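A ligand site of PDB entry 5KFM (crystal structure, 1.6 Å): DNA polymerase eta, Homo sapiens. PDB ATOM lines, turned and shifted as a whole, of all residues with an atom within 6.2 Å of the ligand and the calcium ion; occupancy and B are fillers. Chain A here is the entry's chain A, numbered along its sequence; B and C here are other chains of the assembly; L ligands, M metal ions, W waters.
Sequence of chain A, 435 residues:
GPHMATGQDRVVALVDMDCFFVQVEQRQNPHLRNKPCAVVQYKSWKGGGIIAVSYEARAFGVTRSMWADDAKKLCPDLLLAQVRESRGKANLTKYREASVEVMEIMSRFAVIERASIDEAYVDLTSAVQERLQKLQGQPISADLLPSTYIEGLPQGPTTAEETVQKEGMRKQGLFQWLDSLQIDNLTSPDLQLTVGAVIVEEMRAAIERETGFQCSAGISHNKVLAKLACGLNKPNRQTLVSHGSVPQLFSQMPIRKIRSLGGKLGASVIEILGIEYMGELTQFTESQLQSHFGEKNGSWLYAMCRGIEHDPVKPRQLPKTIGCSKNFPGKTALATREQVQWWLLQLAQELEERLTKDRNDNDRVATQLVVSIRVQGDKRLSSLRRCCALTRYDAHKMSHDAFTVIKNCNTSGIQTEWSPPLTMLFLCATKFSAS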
ATOM      1  N   ASP A  16      12.136   7.893 -25.000  1.00  0.00           N
ATOM      2  CA  ASP A  16      11.016   7.460 -24.167  1.00  0.00           C
ATOM      3  C   ASP A  16       9.694   7.631 -24.945  1.00  0.00           C
ATOM      4  O   ASP A  16       9.270   8.769 -25.189  1.00  0.00           O
ATOM      5  CB  ASP A  16      11.010   8.309 -22.880  1.00  0.00           C
ATOM      6  CG  ASP A  16       9.950   7.905 -21.883  1.00  0.00           C
ATOM      7  OD1 ASP A  16       9.997   8.453 -20.754  1.00  0.00           O
ATOM      8  OD2 ASP A  16       9.085   7.080 -22.203  1.00  0.00           O
ATOM      9  N   MET A  17       9.053   6.551 -25.323  1.00  0.00           N
ATOM     10  CA  MET A  17       7.853   6.695 -26.134  1.00  0.00           C
ATOM     11  C   MET A  17       6.743   7.417 -25.378  1.00  0.00           C
ATOM     12  O   MET A  17       6.627   7.247 -24.244  1.00  0.00           O
ATOM     13  CB  MET A  17       7.315   5.343 -26.612  1.00  0.00           C
ATOM     14  CG  MET A  17       8.339   4.458 -27.284  1.00  0.00           C
ATOM     15  SD  MET A  17       9.059   5.156 -28.803  1.00  0.00           S
ATOM     16  CE  MET A  17       7.640   5.159 -29.854  1.00  0.00           C
ATOM     17  N   ASP A  18       5.947   8.219 -26.065  1.00  0.00           N
ATOM     18  CA  ASP A  18       4.883   8.912 -25.383  1.00  0.00           C
ATOM     19  C   ASP A  18       3.671   7.996 -25.217  1.00  0.00           C
ATOM     20  O   ASP A  18       3.374   7.266 -26.113  1.00  0.00           O
ATOM     21  CB  ASP A  18       4.431  10.120 -26.163  1.00  0.00           C
ATOM     22  CG  ASP A  18       5.523  11.141 -26.361  1.00  0.00           C
ATOM     23  OD1 ASP A  18       6.318  11.307 -25.522  1.00  0.00           O
ATOM     24  OD2 ASP A  18       5.494  11.798 -27.352  1.00  0.00           O
ATOM     25  N   CYS A  19       3.123   7.989 -24.021  1.00  0.00           N
ATOM     26  CA  CYS A  19       1.904   7.286 -23.685  1.00  0.00           C
ATOM     27  C   CYS A  19       1.812   5.932 -24.392  1.00  0.00           C
ATOM     28  O   CYS A  19       0.935   5.709 -25.111  1.00  0.00           O
ATOM     29  CB  CYS A  19       0.634   8.096 -23.737  1.00  0.00           C
ATOM     30  SG  CYS A  19       0.208   8.896 -25.275  1.00  0.00           S
ATOM     31  N   PHE A  20       2.842   5.127 -24.249  1.00  0.00           N
ATOM     32  CA  PHE A  20       3.106   4.103 -25.239  1.00  0.00           C
ATOM     33  C   PHE A  20       2.016   3.080 -25.451  1.00  0.00           C
ATOM     34  O   PHE A  20       1.653   2.906 -26.531  1.00  0.00           O
ATOM     35  CB  PHE A  20       4.365   3.356 -24.835  1.00  0.00           C
ATOM     36  CG  PHE A  20       4.806   2.329 -25.788  1.00  0.00           C
ATOM     37  CD1 PHE A  20       4.956   2.616 -27.085  1.00  0.00           C
ATOM     38  CD2 PHE A  20       5.053   1.051 -25.377  1.00  0.00           C
ATOM     39  CE1 PHE A  20       5.365   1.680 -27.984  1.00  0.00           C
ATOM     40  CE2 PHE A  20       5.460   0.098 -26.280  1.00  0.00           C
ATOM     41  CZ  PHE A  20       5.632   0.433 -27.565  1.00  0.00           C
ATOM     42  N   PHE A  21       1.456   2.470 -24.421  1.00  0.00           N
ATOM     43  CA  PHE A  21       0.407   1.471 -24.698  1.00  0.00           C
ATOM     44  C   PHE A  21      -0.801   2.138 -25.373  1.00  0.00           C
ATOM     45  O   PHE A  21      -1.466   1.524 -26.205  1.00  0.00           O
ATOM     46  CB  PHE A  21      -0.074   0.734 -23.436  1.00  0.00           C
ATOM     47  CG  PHE A  21       0.932  -0.225 -22.829  1.00  0.00           C
ATOM     48  CD1 PHE A  21       2.259  -0.262 -23.229  1.00  0.00           C
ATOM     49  CD2 PHE A  21       0.533  -1.107 -21.836  1.00  0.00           C
ATOM     50  CE1 PHE A  21       3.161  -1.151 -22.671  1.00  0.00           C
ATOM     51  CE2 PHE A  21       1.432  -2.003 -21.271  1.00  0.00           C
ATOM     52  CZ  PHE A  21       2.728  -2.021 -21.676  1.00  0.00           C
ATOM     53  N   VAL A  22      -1.084   3.389 -24.990  1.00  0.00           N
ATOM     54  CA  VAL A  22      -2.130   4.151 -25.650  1.00  0.00           C
ATOM     55  C   VAL A  22      -1.842   4.296 -27.136  1.00  0.00           C
ATOM     56  O   VAL A  22      -2.726   4.039 -27.979  1.00  0.00           O
ATOM     57  CB  VAL A  22      -2.312   5.543 -25.018  1.00  0.00           C
ATOM     58  CG1 VAL A  22      -3.081   6.477 -25.972  1.00  0.00           C
ATOM     59  CG2 VAL A  22      -3.075   5.416 -23.720  1.00  0.00           C
ATOM     60  N   GLN A  41      -6.513  -2.836 -17.649  1.00  0.00           N
ATOM     61  CA  GLN A  41      -6.458  -4.292 -17.641  1.00  0.00           C
ATOM     62  C   GLN A  41      -7.519  -4.805 -16.696  1.00  0.00           C
ATOM     63  O   GLN A  41      -7.697  -4.277 -15.599  1.00  0.00           O
ATOM     64  CB  GLN A  41      -5.081  -4.816 -17.264  1.00  0.00           C
ATOM     65  CG  GLN A  41      -4.464  -4.198 -16.049  1.00  0.00           C
ATOM     66  CD  GLN A  41      -3.030  -4.647 -15.856  1.00  0.00           C
ATOM     67  OE1 GLN A  41      -2.456  -5.319 -16.727  1.00  0.00           O
ATOM     68  NE2 GLN A  41      -2.441  -4.289 -14.724  1.00  0.00           N
ATOM     69  N   ILE A  51      -3.465   1.562 -16.839  1.00  0.00           N
ATOM     70  CA  ILE A  51      -2.009   1.501 -16.872  1.00  0.00           C
ATOM     71  C   ILE A  51      -1.368   2.481 -17.851  1.00  0.00           C
ATOM     72  O   ILE A  51      -0.157   2.634 -17.845  1.00  0.00           O
ATOM     73  CB  ILE A  51      -1.491   0.083 -17.191  1.00  0.00           C
ATOM     74  CG1 ILE A  51      -1.996  -0.418 -18.545  1.00  0.00           C
ATOM     75  CG2 ILE A  51      -1.876  -0.903 -16.050  1.00  0.00           C
ATOM     76  CD1 ILE A  51      -1.407  -1.771 -18.922  1.00  0.00           C
ATOM     77  N   ALA A  52      -2.175   3.136 -18.691  1.00  0.00           N
ATOM     78  CA  ALA A  52      -1.640   4.160 -19.615  1.00  0.00           C
ATOM     79  C   ALA A  52      -2.715   5.165 -19.976  1.00  0.00           C
ATOM     80  O   ALA A  52      -3.887   4.817 -20.082  1.00  0.00           O
ATOM     81  CB  ALA A  52      -1.054   3.506 -20.887  1.00  0.00           C
ATOM     82  N   VAL A  53      -2.310   6.422 -20.162  1.00  0.00           N
ATOM     83  CA  VAL A  53      -3.239   7.543 -20.332  1.00  0.00           C
ATOM     84  C   VAL A  53      -2.770   8.508 -21.410  1.00  0.00           C
ATOM     85  O   VAL A  53      -1.630   8.984 -21.374  1.00  0.00           O
ATOM     86  CB  VAL A  53      -3.379   8.354 -19.009  1.00  0.00           C
ATOM     87  CG1 VAL A  53      -4.501   9.340 -19.113  1.00  0.00           C
ATOM     88  CG2 VAL A  53      -3.630   7.414 -17.824  1.00  0.00           C
ATOM     89  N   TYR A  55      -2.532  12.072 -23.461  1.00  0.00           N
ATOM     90  CA  TYR A  55      -2.352  13.408 -22.920  1.00  0.00           C
ATOM     91  C   TYR A  55      -3.670  14.184 -22.876  1.00  0.00           C
ATOM     92  O   TYR A  55      -3.887  14.968 -21.954  1.00  0.00           O
ATOM     93  CB  TYR A  55      -1.249  14.155 -23.701  1.00  0.00           C
ATOM     94  CG  TYR A  55       0.123  13.680 -23.262  1.00  0.00           C
ATOM     95  CD1 TYR A  55       0.651  12.477 -23.739  1.00  0.00           C
ATOM     96  CD2 TYR A  55       0.857  14.377 -22.309  1.00  0.00           C
ATOM     97  CE1 TYR A  55       1.888  12.009 -23.306  1.00  0.00           C
ATOM     98  CE2 TYR A  55       2.097  13.925 -21.872  1.00  0.00           C
ATOM     99  CZ  TYR A  55       2.615  12.739 -22.364  1.00  0.00           C
ATOM    100  OH  TYR A  55       3.832  12.279 -21.929  1.00  0.00           O
ATOM    101  N   ARG A  58      -5.099  13.106 -19.684  1.00  0.00           N
ATOM    102  CA  ARG A  58      -4.364  13.621 -18.537  1.00  0.00           C
ATOM    103  C   ARG A  58      -4.856  15.019 -18.171  1.00  0.00           C
ATOM    104  O   ARG A  58      -4.820  15.392 -16.991  1.00  0.00           O
ATOM    105  CB  ARG A  58      -2.861  13.656 -18.823  1.00  0.00           C
ATOM    106  CG  ARG A  58      -2.260  12.274 -18.977  1.00  0.00           C
ATOM    107  CD  ARG A  58      -0.773  12.305 -19.257  1.00  0.00           C
ATOM    108  NE  ARG A  58      -0.363  11.022 -19.795  1.00  0.00           N
ATOM    109  CZ  ARG A  58       0.881  10.585 -19.883  1.00  0.00           C
ATOM    110  NH1 ARG A  58       1.884  11.351 -19.477  1.00  0.00           N
ATOM    111  NH2 ARG A  58       1.114   9.375 -20.399  1.00  0.00           N
ATOM    112  N   ARG A  64      -2.424   6.893 -14.269  1.00  0.00           N
ATOM    113  CA  ARG A  64      -2.128   5.482 -14.008  1.00  0.00           C
ATOM    114  C   ARG A  64      -2.544   5.131 -12.581  1.00  0.00           C
ATOM    115  O   ARG A  64      -2.541   6.008 -11.715  1.00  0.00           O
ATOM    116  CB  ARG A  64      -0.644   5.197 -14.231  1.00  0.00           C
ATOM    117  CG  ARG A  64      -0.142   3.859 -13.743  1.00  0.00           C
ATOM    118  CD  ARG A  64       1.289   3.631 -14.173  1.00  0.00           C
ATOM    119  NE  ARG A  64       1.397   3.684 -15.634  1.00  0.00           N
ATOM    120  CZ  ARG A  64       2.022   4.641 -16.305  1.00  0.00           C
ATOM    121  NH1 ARG A  64       2.628   5.625 -15.656  1.00  0.00           N
ATOM    122  NH2 ARG A  64       2.033   4.612 -17.632  1.00  0.00           N
ATOM    123  N   SER A 116      13.509  -0.179 -20.480  1.00  0.00           N
ATOM    124  CA  SER A 116      12.202  -0.647 -20.107  1.00  0.00           C
ATOM    125  C   SER A 116      11.479  -0.995 -21.387  1.00  0.00           C
ATOM    126  O   SER A 116      12.080  -1.015 -22.463  1.00  0.00           O
ATOM    127  CB  SER A 116      11.419   0.421 -19.335  1.00  0.00           C
ATOM    128  OG  SER A 116      11.112   1.511 -20.190  1.00  0.00           O
ATOM    129  N   ILE A 117      10.176  -1.265 -21.293  1.00  0.00           N
ATOM    130  CA  ILE A 117       9.432  -1.659 -22.467  1.00  0.00           C
ATOM    131  C   ILE A 117       9.411  -0.572 -23.556  1.00  0.00           C
ATOM    132  O   ILE A 117       9.308  -0.874 -24.730  1.00  0.00           O
ATOM    133  CB  ILE A 117       7.987  -2.052 -22.088  1.00  0.00           C
ATOM    134  CG1 ILE A 117       7.350  -2.845 -23.241  1.00  0.00           C
ATOM    135  CG2 ILE A 117       7.174  -0.818 -21.668  1.00  0.00           C
ATOM    136  CD1 ILE A 117       6.127  -3.654 -22.853  1.00  0.00           C
ATOM    137  N   ASP A 118       9.588   0.695 -23.175  1.00  0.00           N
ATOM    138  CA  ASP A 118       9.465   1.759 -24.175  1.00  0.00           C
ATOM    139  C   ASP A 118      10.521   2.852 -24.048  1.00  0.00           C
ATOM    140  O   ASP A 118      10.315   3.983 -24.508  1.00  0.00           O
ATOM    141  CB  ASP A 118       8.070   2.379 -24.094  1.00  0.00           C
ATOM    142  CG  ASP A 118       7.928   3.348 -22.932  1.00  0.00           C
ATOM    143  OD1 ASP A 118       7.167   4.312 -23.063  1.00  0.00           O
ATOM    144  OD2 ASP A 118       8.585   3.151 -21.891  1.00  0.00           O
ATOM    145  N   GLU A 119      11.627   2.501 -23.404  1.00  0.00           N
ATOM    146  CA  GLU A 119      12.737   3.424 -23.157  1.00  0.00           C
ATOM    147  C   GLU A 119      14.048   2.767 -23.520  1.00  0.00           C
ATOM    148  O   GLU A 119      14.247   1.577 -23.239  1.00  0.00           O
ATOM    149  CB  GLU A 119      12.817   3.851 -21.689  1.00  0.00           C
ATOM    150  CG  GLU A 119      11.612   4.601 -21.138  1.00  0.00           C
ATOM    151  CD  GLU A 119      11.789   4.942 -19.655  1.00  0.00           C
ATOM    152  OE1 GLU A 119      12.750   4.412 -19.063  1.00  0.00           O
ATOM    153  OE2 GLU A 119      10.983   5.725 -19.107  1.00  0.00           O
ATOM    154  N   LYS A 227      17.943  11.215 -19.094  1.00  0.00           N
ATOM    155  CA  LYS A 227      16.624  10.823 -18.617  1.00  0.00           C
ATOM    156  C   LYS A 227      15.866  12.039 -18.067  1.00  0.00           C
ATOM    157  O   LYS A 227      14.707  12.256 -18.411  1.00  0.00           O
ATOM    158  CB  LYS A 227      16.749   9.735 -17.554  1.00  0.00           C
ATOM    159  CG  LYS A 227      15.438   9.384 -16.873  1.00  0.00           C
ATOM    160  CD  LYS A 227      14.400   8.927 -17.866  1.00  0.00           C
ATOM    161  CE  LYS A 227      13.126   8.477 -17.171  1.00  0.00           C
ATOM    162  NZ  LYS A 227      12.033   8.261 -18.155  1.00  0.00           N
ATOM    163  N   LYS A 234       8.183  16.586 -22.631  1.00  0.00           N
ATOM    164  CA  LYS A 234       7.189  15.616 -23.097  1.00  0.00           C
ATOM    165  C   LYS A 234       5.853  16.314 -23.341  1.00  0.00           C
ATOM    166  O   LYS A 234       5.502  17.214 -22.577  1.00  0.00           O
ATOM    167  CB  LYS A 234       6.971  14.498 -22.068  1.00  0.00           C
ATOM    168  CG  LYS A 234       7.771  13.247 -22.275  1.00  0.00           C
ATOM    169  CD  LYS A 234       7.177  12.052 -21.515  1.00  0.00           C
ATOM    170  CE  LYS A 234       7.916  10.766 -21.879  1.00  0.00           C
ATOM    171  NZ  LYS A 234       7.510  10.223 -23.231  1.00  0.00           N
ATOM    172  N   PRO A 235       5.077  15.887 -24.353  1.00  0.00           N
ATOM    173  CA  PRO A 235       5.390  14.849 -25.343  1.00  0.00           C
ATOM    174  C   PRO A 235       5.868  15.390 -26.673  1.00  0.00           C
ATOM    175  O   PRO A 235       5.771  16.595 -26.938  1.00  0.00           O
ATOM    176  CB  PRO A 235       4.040  14.173 -25.545  1.00  0.00           C
ATOM    177  CG  PRO A 235       3.093  15.361 -25.492  1.00  0.00           C
ATOM    178  CD  PRO A 235       3.655  16.263 -24.398  1.00  0.00           C
ATOM    179  P    DT B   3      -5.934  -0.973  -3.942  1.00  0.00           P
ATOM    180  OP1  DT B   3      -5.706  -1.176  -2.500  1.00  0.00           O
ATOM    181  OP2  DT B   3      -6.693   0.205  -4.424  1.00  0.00           O
ATOM    182  O5'  DT B   3      -4.520  -0.986  -4.685  1.00  0.00           O
ATOM    183  C5'  DT B   3      -4.388  -0.475  -6.008  1.00  0.00           C
ATOM    184  C4'  DT B   3      -4.694  -1.544  -7.031  1.00  0.00           C
ATOM    185  O4'  DT B   3      -4.415  -1.022  -8.356  1.00  0.00           O
ATOM    186  C3'  DT B   3      -3.880  -2.823  -6.897  1.00  0.00           C
ATOM    187  O3'  DT B   3      -4.626  -3.929  -7.350  1.00  0.00           O
ATOM    188  C2'  DT B   3      -2.707  -2.542  -7.825  1.00  0.00           C
ATOM    189  C1'  DT B   3      -3.384  -1.793  -8.952  1.00  0.00           C
ATOM    190  N1   DT B   3      -2.471  -0.870  -9.671  1.00  0.00           N
ATOM    191  C2   DT B   3      -2.517  -0.814 -11.045  1.00  0.00           C
ATOM    192  O2   DT B   3      -3.288  -1.470 -11.720  1.00  0.00           O
ATOM    193  N3   DT B   3      -1.629   0.070 -11.607  1.00  0.00           N
ATOM    194  C4   DT B   3      -0.712   0.872 -10.944  1.00  0.00           C
ATOM    195  O4   DT B   3       0.040   1.636 -11.538  1.00  0.00           O
ATOM    196  C5   DT B   3      -0.715   0.751  -9.505  1.00  0.00           C
ATOM    197  C7   DT B   3       0.223   1.569  -8.672  1.00  0.00           C
ATOM    198  C6   DT B   3      -1.588  -0.099  -8.947  1.00  0.00           C
ATOM    199  P    DT B   4      -3.944  -5.370  -7.482  1.00  0.00           P
ATOM    200  OP1  DT B   4      -5.026  -6.384  -7.419  1.00  0.00           O
ATOM    201  OP2  DT B   4      -2.792  -5.430  -6.542  1.00  0.00           O
ATOM    202  O5'  DT B   4      -3.349  -5.393  -8.957  1.00  0.00           O
ATOM    203  C5'  DT B   4      -4.236  -5.510 -10.053  1.00  0.00           C
ATOM    204  C4'  DT B   4      -3.498  -5.936 -11.309  1.00  0.00           C
ATOM    205  O4'  DT B   4      -2.606  -4.882 -11.740  1.00  0.00           O
ATOM    206  C3'  DT B   4      -2.632  -7.176 -11.178  1.00  0.00           C
ATOM    207  O3'  DT B   4      -2.673  -7.864 -12.418  1.00  0.00           O
ATOM    208  C2'  DT B   4      -1.242  -6.578 -10.896  1.00  0.00           C
ATOM    209  C1'  DT B   4      -1.278  -5.365 -11.820  1.00  0.00           C
ATOM    210  N1   DT B   4      -0.392  -4.233 -11.472  1.00  0.00           N
ATOM    211  C2   DT B   4       0.128  -3.491 -12.498  1.00  0.00           C
ATOM    212  O2   DT B   4      -0.059  -3.775 -13.663  1.00  0.00           O
ATOM    213  N3   DT B   4       0.880  -2.436 -12.124  1.00  0.00           N
ATOM    214  C4   DT B   4       1.169  -2.013 -10.844  1.00  0.00           C
ATOM    215  O4   DT B   4       1.858  -1.031 -10.622  1.00  0.00           O
ATOM    216  C5   DT B   4       0.562  -2.807  -9.782  1.00  0.00           C
ATOM    217  C7   DT B   4       0.820  -2.448  -8.342  1.00  0.00           C
ATOM    218  C6   DT B   4      -0.186  -3.866 -10.143  1.00  0.00           C
ATOM    219  P    DA B   5      -1.889  -9.255 -12.656  1.00  0.00           P
ATOM    220  OP1  DA B   5      -2.788 -10.129 -13.417  1.00  0.00           O
ATOM    221  OP2  DA B   5      -1.259  -9.720 -11.386  1.00  0.00           O
ATOM    222  O5'  DA B   5      -0.685  -8.822 -13.594  1.00  0.00           O
ATOM    223  C5'  DA B   5      -0.948  -8.407 -14.933  1.00  0.00           C
ATOM    224  C4'  DA B   5       0.361  -8.100 -15.602  1.00  0.00           C
ATOM    225  O4'  DA B   5       0.904  -6.902 -14.987  1.00  0.00           O
ATOM    226  C3'  DA B   5       1.437  -9.183 -15.450  1.00  0.00           C
ATOM    227  O3'  DA B   5       2.115  -9.346 -16.690  1.00  0.00           O
ATOM    228  C2'  DA B   5       2.357  -8.604 -14.369  1.00  0.00           C
ATOM    229  C1'  DA B   5       2.268  -7.137 -14.699  1.00  0.00           C
ATOM    230  N9   DA B   5       2.685  -6.248 -13.621  1.00  0.00           N
ATOM    231  C8   DA B   5       2.435  -6.395 -12.284  1.00  0.00           C
ATOM    232  N7   DA B   5       2.923  -5.413 -11.556  1.00  0.00           N
ATOM    233  C5   DA B   5       3.525  -4.573 -12.485  1.00  0.00           C
ATOM    234  C6   DA B   5       4.218  -3.364 -12.353  1.00  0.00           C
ATOM    235  N6   DA B   5       4.436  -2.765 -11.178  1.00  0.00           N
ATOM    236  N1   DA B   5       4.681  -2.789 -13.479  1.00  0.00           N
ATOM    237  C2   DA B   5       4.462  -3.388 -14.654  1.00  0.00           C
ATOM    238  N3   DA B   5       3.829  -4.537 -14.897  1.00  0.00           N
ATOM    239  C4   DA B   5       3.379  -5.075 -13.758  1.00  0.00           C
ATOM    240  P    DT C   8      10.059   5.355 -14.190  1.00  0.00           P
ATOM    241  OP1  DT C   8      10.467   6.578 -14.922  1.00  0.00           O
ATOM    242  OP2  DT C   8       8.954   5.420 -13.197  1.00  0.00           O
ATOM    243  O5'  DT C   8       9.671   4.118 -15.162  1.00  0.00           O
ATOM    244  C5'  DT C   8      10.338   3.928 -16.405  1.00  0.00           C
ATOM    245  C4'  DT C   8       9.815   2.691 -17.141  1.00  0.00           C
ATOM    246  O4'  DT C   8       9.504   1.638 -16.206  1.00  0.00           O
ATOM    247  C3'  DT C   8       8.558   2.890 -18.001  1.00  0.00           C
ATOM    248  O3'  DT C   8       8.732   2.256 -19.250  1.00  0.00           O
ATOM    249  C2'  DT C   8       7.454   2.232 -17.188  1.00  0.00           C
ATOM    250  C1'  DT C   8       8.202   1.147 -16.440  1.00  0.00           C
ATOM    251  N1   DT C   8       7.570   0.806 -15.143  1.00  0.00           N
ATOM    252  C2   DT C   8       6.794  -0.327 -15.048  1.00  0.00           C
ATOM    253  O2   DT C   8       6.591  -1.079 -15.979  1.00  0.00           O
ATOM    254  N3   DT C   8       6.264  -0.555 -13.808  1.00  0.00           N
ATOM    255  C4   DT C   8       6.409   0.229 -12.687  1.00  0.00           C
ATOM    256  O4   DT C   8       5.891  -0.063 -11.612  1.00  0.00           O
ATOM    257  C5   DT C   8       7.217   1.412 -12.853  1.00  0.00           C
ATOM    258  C7   DT C   8       7.450   2.339 -11.689  1.00  0.00           C
ATOM    259  C6   DT C   8       7.758   1.642 -14.057  1.00  0.00           C
HETATM  260  P1  LIG L   1       4.722   8.969 -20.904  1.00  0.00           P
HETATM  261  O1  LIG L   1       6.046   8.289 -21.098  1.00  0.00           O
HETATM  262  O2  LIG L   1       4.343   9.798 -22.091  1.00  0.00           O
HETATM  263  O3  LIG L   1       4.652   9.764 -19.591  1.00  0.00           O
HETATM  264  P2  LIG L   1       3.802   6.276 -20.764  1.00  0.00           P
HETATM  265  O4  LIG L   1       4.664   5.860 -21.942  1.00  0.00           O
HETATM  266  O5  LIG L   1       2.444   5.608 -20.873  1.00  0.00           O
HETATM  267  O6  LIG L   1       3.555   7.869 -20.751  1.00  0.00           O
HETATM  268  P3  LIG L   1       5.744   5.152 -18.953  1.00  0.00           P
HETATM  269  S1  LIG L   1       6.013   5.497 -17.057  1.00  0.00           S
HETATM  270  O7  LIG L   1       6.866   5.566 -19.847  1.00  0.00           O
HETATM  271  O8  LIG L   1       4.403   5.948 -19.319  1.00  0.00           O
HETATM  272  O9  LIG L   1       5.418   3.609 -19.136  1.00  0.00           O
HETATM  273  C1  LIG L   1       5.446   3.001 -20.390  1.00  0.00           C
HETATM  274  C2  LIG L   1       4.380   1.927 -20.515  1.00  0.00           C
HETATM  275  O10 LIG L   1       4.644   0.954 -19.525  1.00  0.00           O
HETATM  276  C3  LIG L   1       3.057   2.459 -20.267  1.00  0.00           C
HETATM  277  O11 LIG L   1       2.437   2.930 -21.485  1.00  0.00           O
HETATM  278  C4  LIG L   1       2.323   1.335 -19.683  1.00  0.00           C
HETATM  279  C5  LIG L   1       3.368   0.572 -18.952  1.00  0.00           C
HETATM  280  N1  LIG L   1       3.394   0.868 -17.561  1.00  0.00           N
HETATM  281  C6  LIG L   1       3.961   1.930 -16.945  1.00  0.00           C
HETATM  282  N2  LIG L   1       3.786   1.858 -15.627  1.00  0.00           N
HETATM  283  C7  LIG L   1       3.100   0.738 -15.345  1.00  0.00           C
HETATM  284  C8  LIG L   1       2.633   0.122 -14.189  1.00  0.00           C
HETATM  285  N3  LIG L   1       2.841   0.694 -12.899  1.00  0.00           N
HETATM  286  N4  LIG L   1       1.974  -1.022 -14.318  1.00  0.00           N
HETATM  287  C9  LIG L   1       1.735  -1.622 -15.500  1.00  0.00           C
HETATM  288  N5  LIG L   1       2.182  -1.064 -16.648  1.00  0.00           N
HETATM  289  C10 LIG L   1       2.850   0.096 -16.574  1.00  0.00           C
HETATM  290 CA    CA M   1       6.942   6.396 -22.061  1.00  0.00          CA
HETATM  291  O   HOH W   1       3.759   3.204 -11.255  1.00  0.00           O
HETATM  292  O   HOH W   2       3.809   8.679 -17.378  1.00  0.00           O
HETATM  293  O   HOH W   3       6.098  -1.445 -18.317  1.00  0.00           O
HETATM  294  O   HOH W   4       8.433   7.534 -18.802  1.00  0.00           O
HETATM  295  O   HOH W   5       0.423   6.800 -19.439  1.00  0.00           O
HETATM  296  O   HOH W   6       6.983   9.561 -18.035  1.00  0.00           O
HETATM  297  O   HOH W   7       2.309  -3.356 -18.374  1.00  0.00           O
HETATM  298  O   HOH W   8       4.408   3.758 -13.571  1.00  0.00           O
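The calcium ion is bound by OD2 of Asp 16, O1 of the ligand, OD1 of Asp 118, O4 of the ligand, O of Met 17 and O7 of the ligand. The calcium ion has six donor atoms within binding distance.
Water W8 bridges a nitrogen (N2) of the ligand (2.9 Å) and the guanidinium group (NH1) of Arg 64 (3.3 Å). Water W3 bridges O2 of DT 8 of chain C and an oxygen (O10) of the ligand.
N1 of DA 5 of chain B sits close to a nitrogen (N4) of the ligand (3.3 Å). Asp 18 touches the ligand (CA to O2, 3.5 Å). Ile 51 touches the ligand (O to C4, 3.3 Å). Ala 52 touches the ligand (CB to O11, 3.6 Å). Ile 117 touches the ligand (CG2 to O10, 3.8 Å). Hydrophobic or aromatic side chains that line the ligand: Phe 20, Phe 21, Ile 51, Ala 52, Tyr 55 and Ile 117. 18 residues have an atom within 4 Å of the ligand: Asp 16, Met 17, Asp 18, Cys 19, Phe 20, Phe 21, Ile 51, Ala 52, Tyr 55, Arg 58, Arg 64, Ile 117, Asp 118, Lys 234, DT 3 of chain B, DT 4 of chain B, DA 5 of chain B and DT 8 of chain C. Along chain A the residues within 4 Å of the ligand span positions 16 to 234.
The backbone NH of Cys 19 lies within hydrogen-bond range of an oxygen (O2) of the ligand, at 2.9 Å. The backbone NH (N) of Phe 20 lies within hydrogen-bond range of an oxygen (O5) of the ligand (3.4 Å). A nitrogen (N3) of the ligand sits at hydrogen-bond distance from O4 of DT 3 of chain B. O3 of the ligand lies within salt-bridge range of NH1 of Arg 58, 3.2 Å away. The backbone NH of Phe 21 lies within hydrogen-bond range of an oxygen (O11) of the ligand, at 3.1 Å. O4 of DT 8 of chain C sits at hydrogen-bond distance from a nitrogen (N3) of the ligand, 3.4 Å away. O4 of DT 4 of chain B sits at hydrogen-bond distance from N3 of the ligand (3.0 Å). O2 of the ligand lies within salt-bridge range of NZ of Lys 234, 3.4 Å away. The side-chain hydroxyl (OH) of Tyr 55 is in hydrogen-bond range of an oxygen (O2) of the ligand. The guanidinium group (NH2) of Arg 64 lies within salt-bridge range of an oxygen (O5) of the ligand (3.4 Å).
Within 4 Å of the calcium ion: Asp 16, Met 17 and Asp 118.
OD1 of Asp 16 is in salt-bridge range of NZ of Lys 234, 3.9 Å away. The side-chain amino group (NZ) of Lys 234 lies close to the backbone carbonyl oxygen (O) of Met 17, at 3.3 Å. O2 of DT 4 of chain B lies within hydrogen-bond range of NE2 of Gln 41 (2.7 Å). OH of Tyr 55 lies within hydrogen-bond range of NH1 of Arg 58. The backbone NH of Asp 118 sits close to the side-chain hydroxyl of Ser 116 (3.4 Å). NZ of Lys 234 lies within salt-bridge range of OD1 of Asp 18. OP1 of DT 8 of chain C is in salt-bridge range of the side-chain amino group of Lys 227, 3.97 Å away. The backbone carbonyl oxygen of Ile 51 lies within hydrogen-bond range of the guanidinium group of Arg 64 (2.9 Å).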
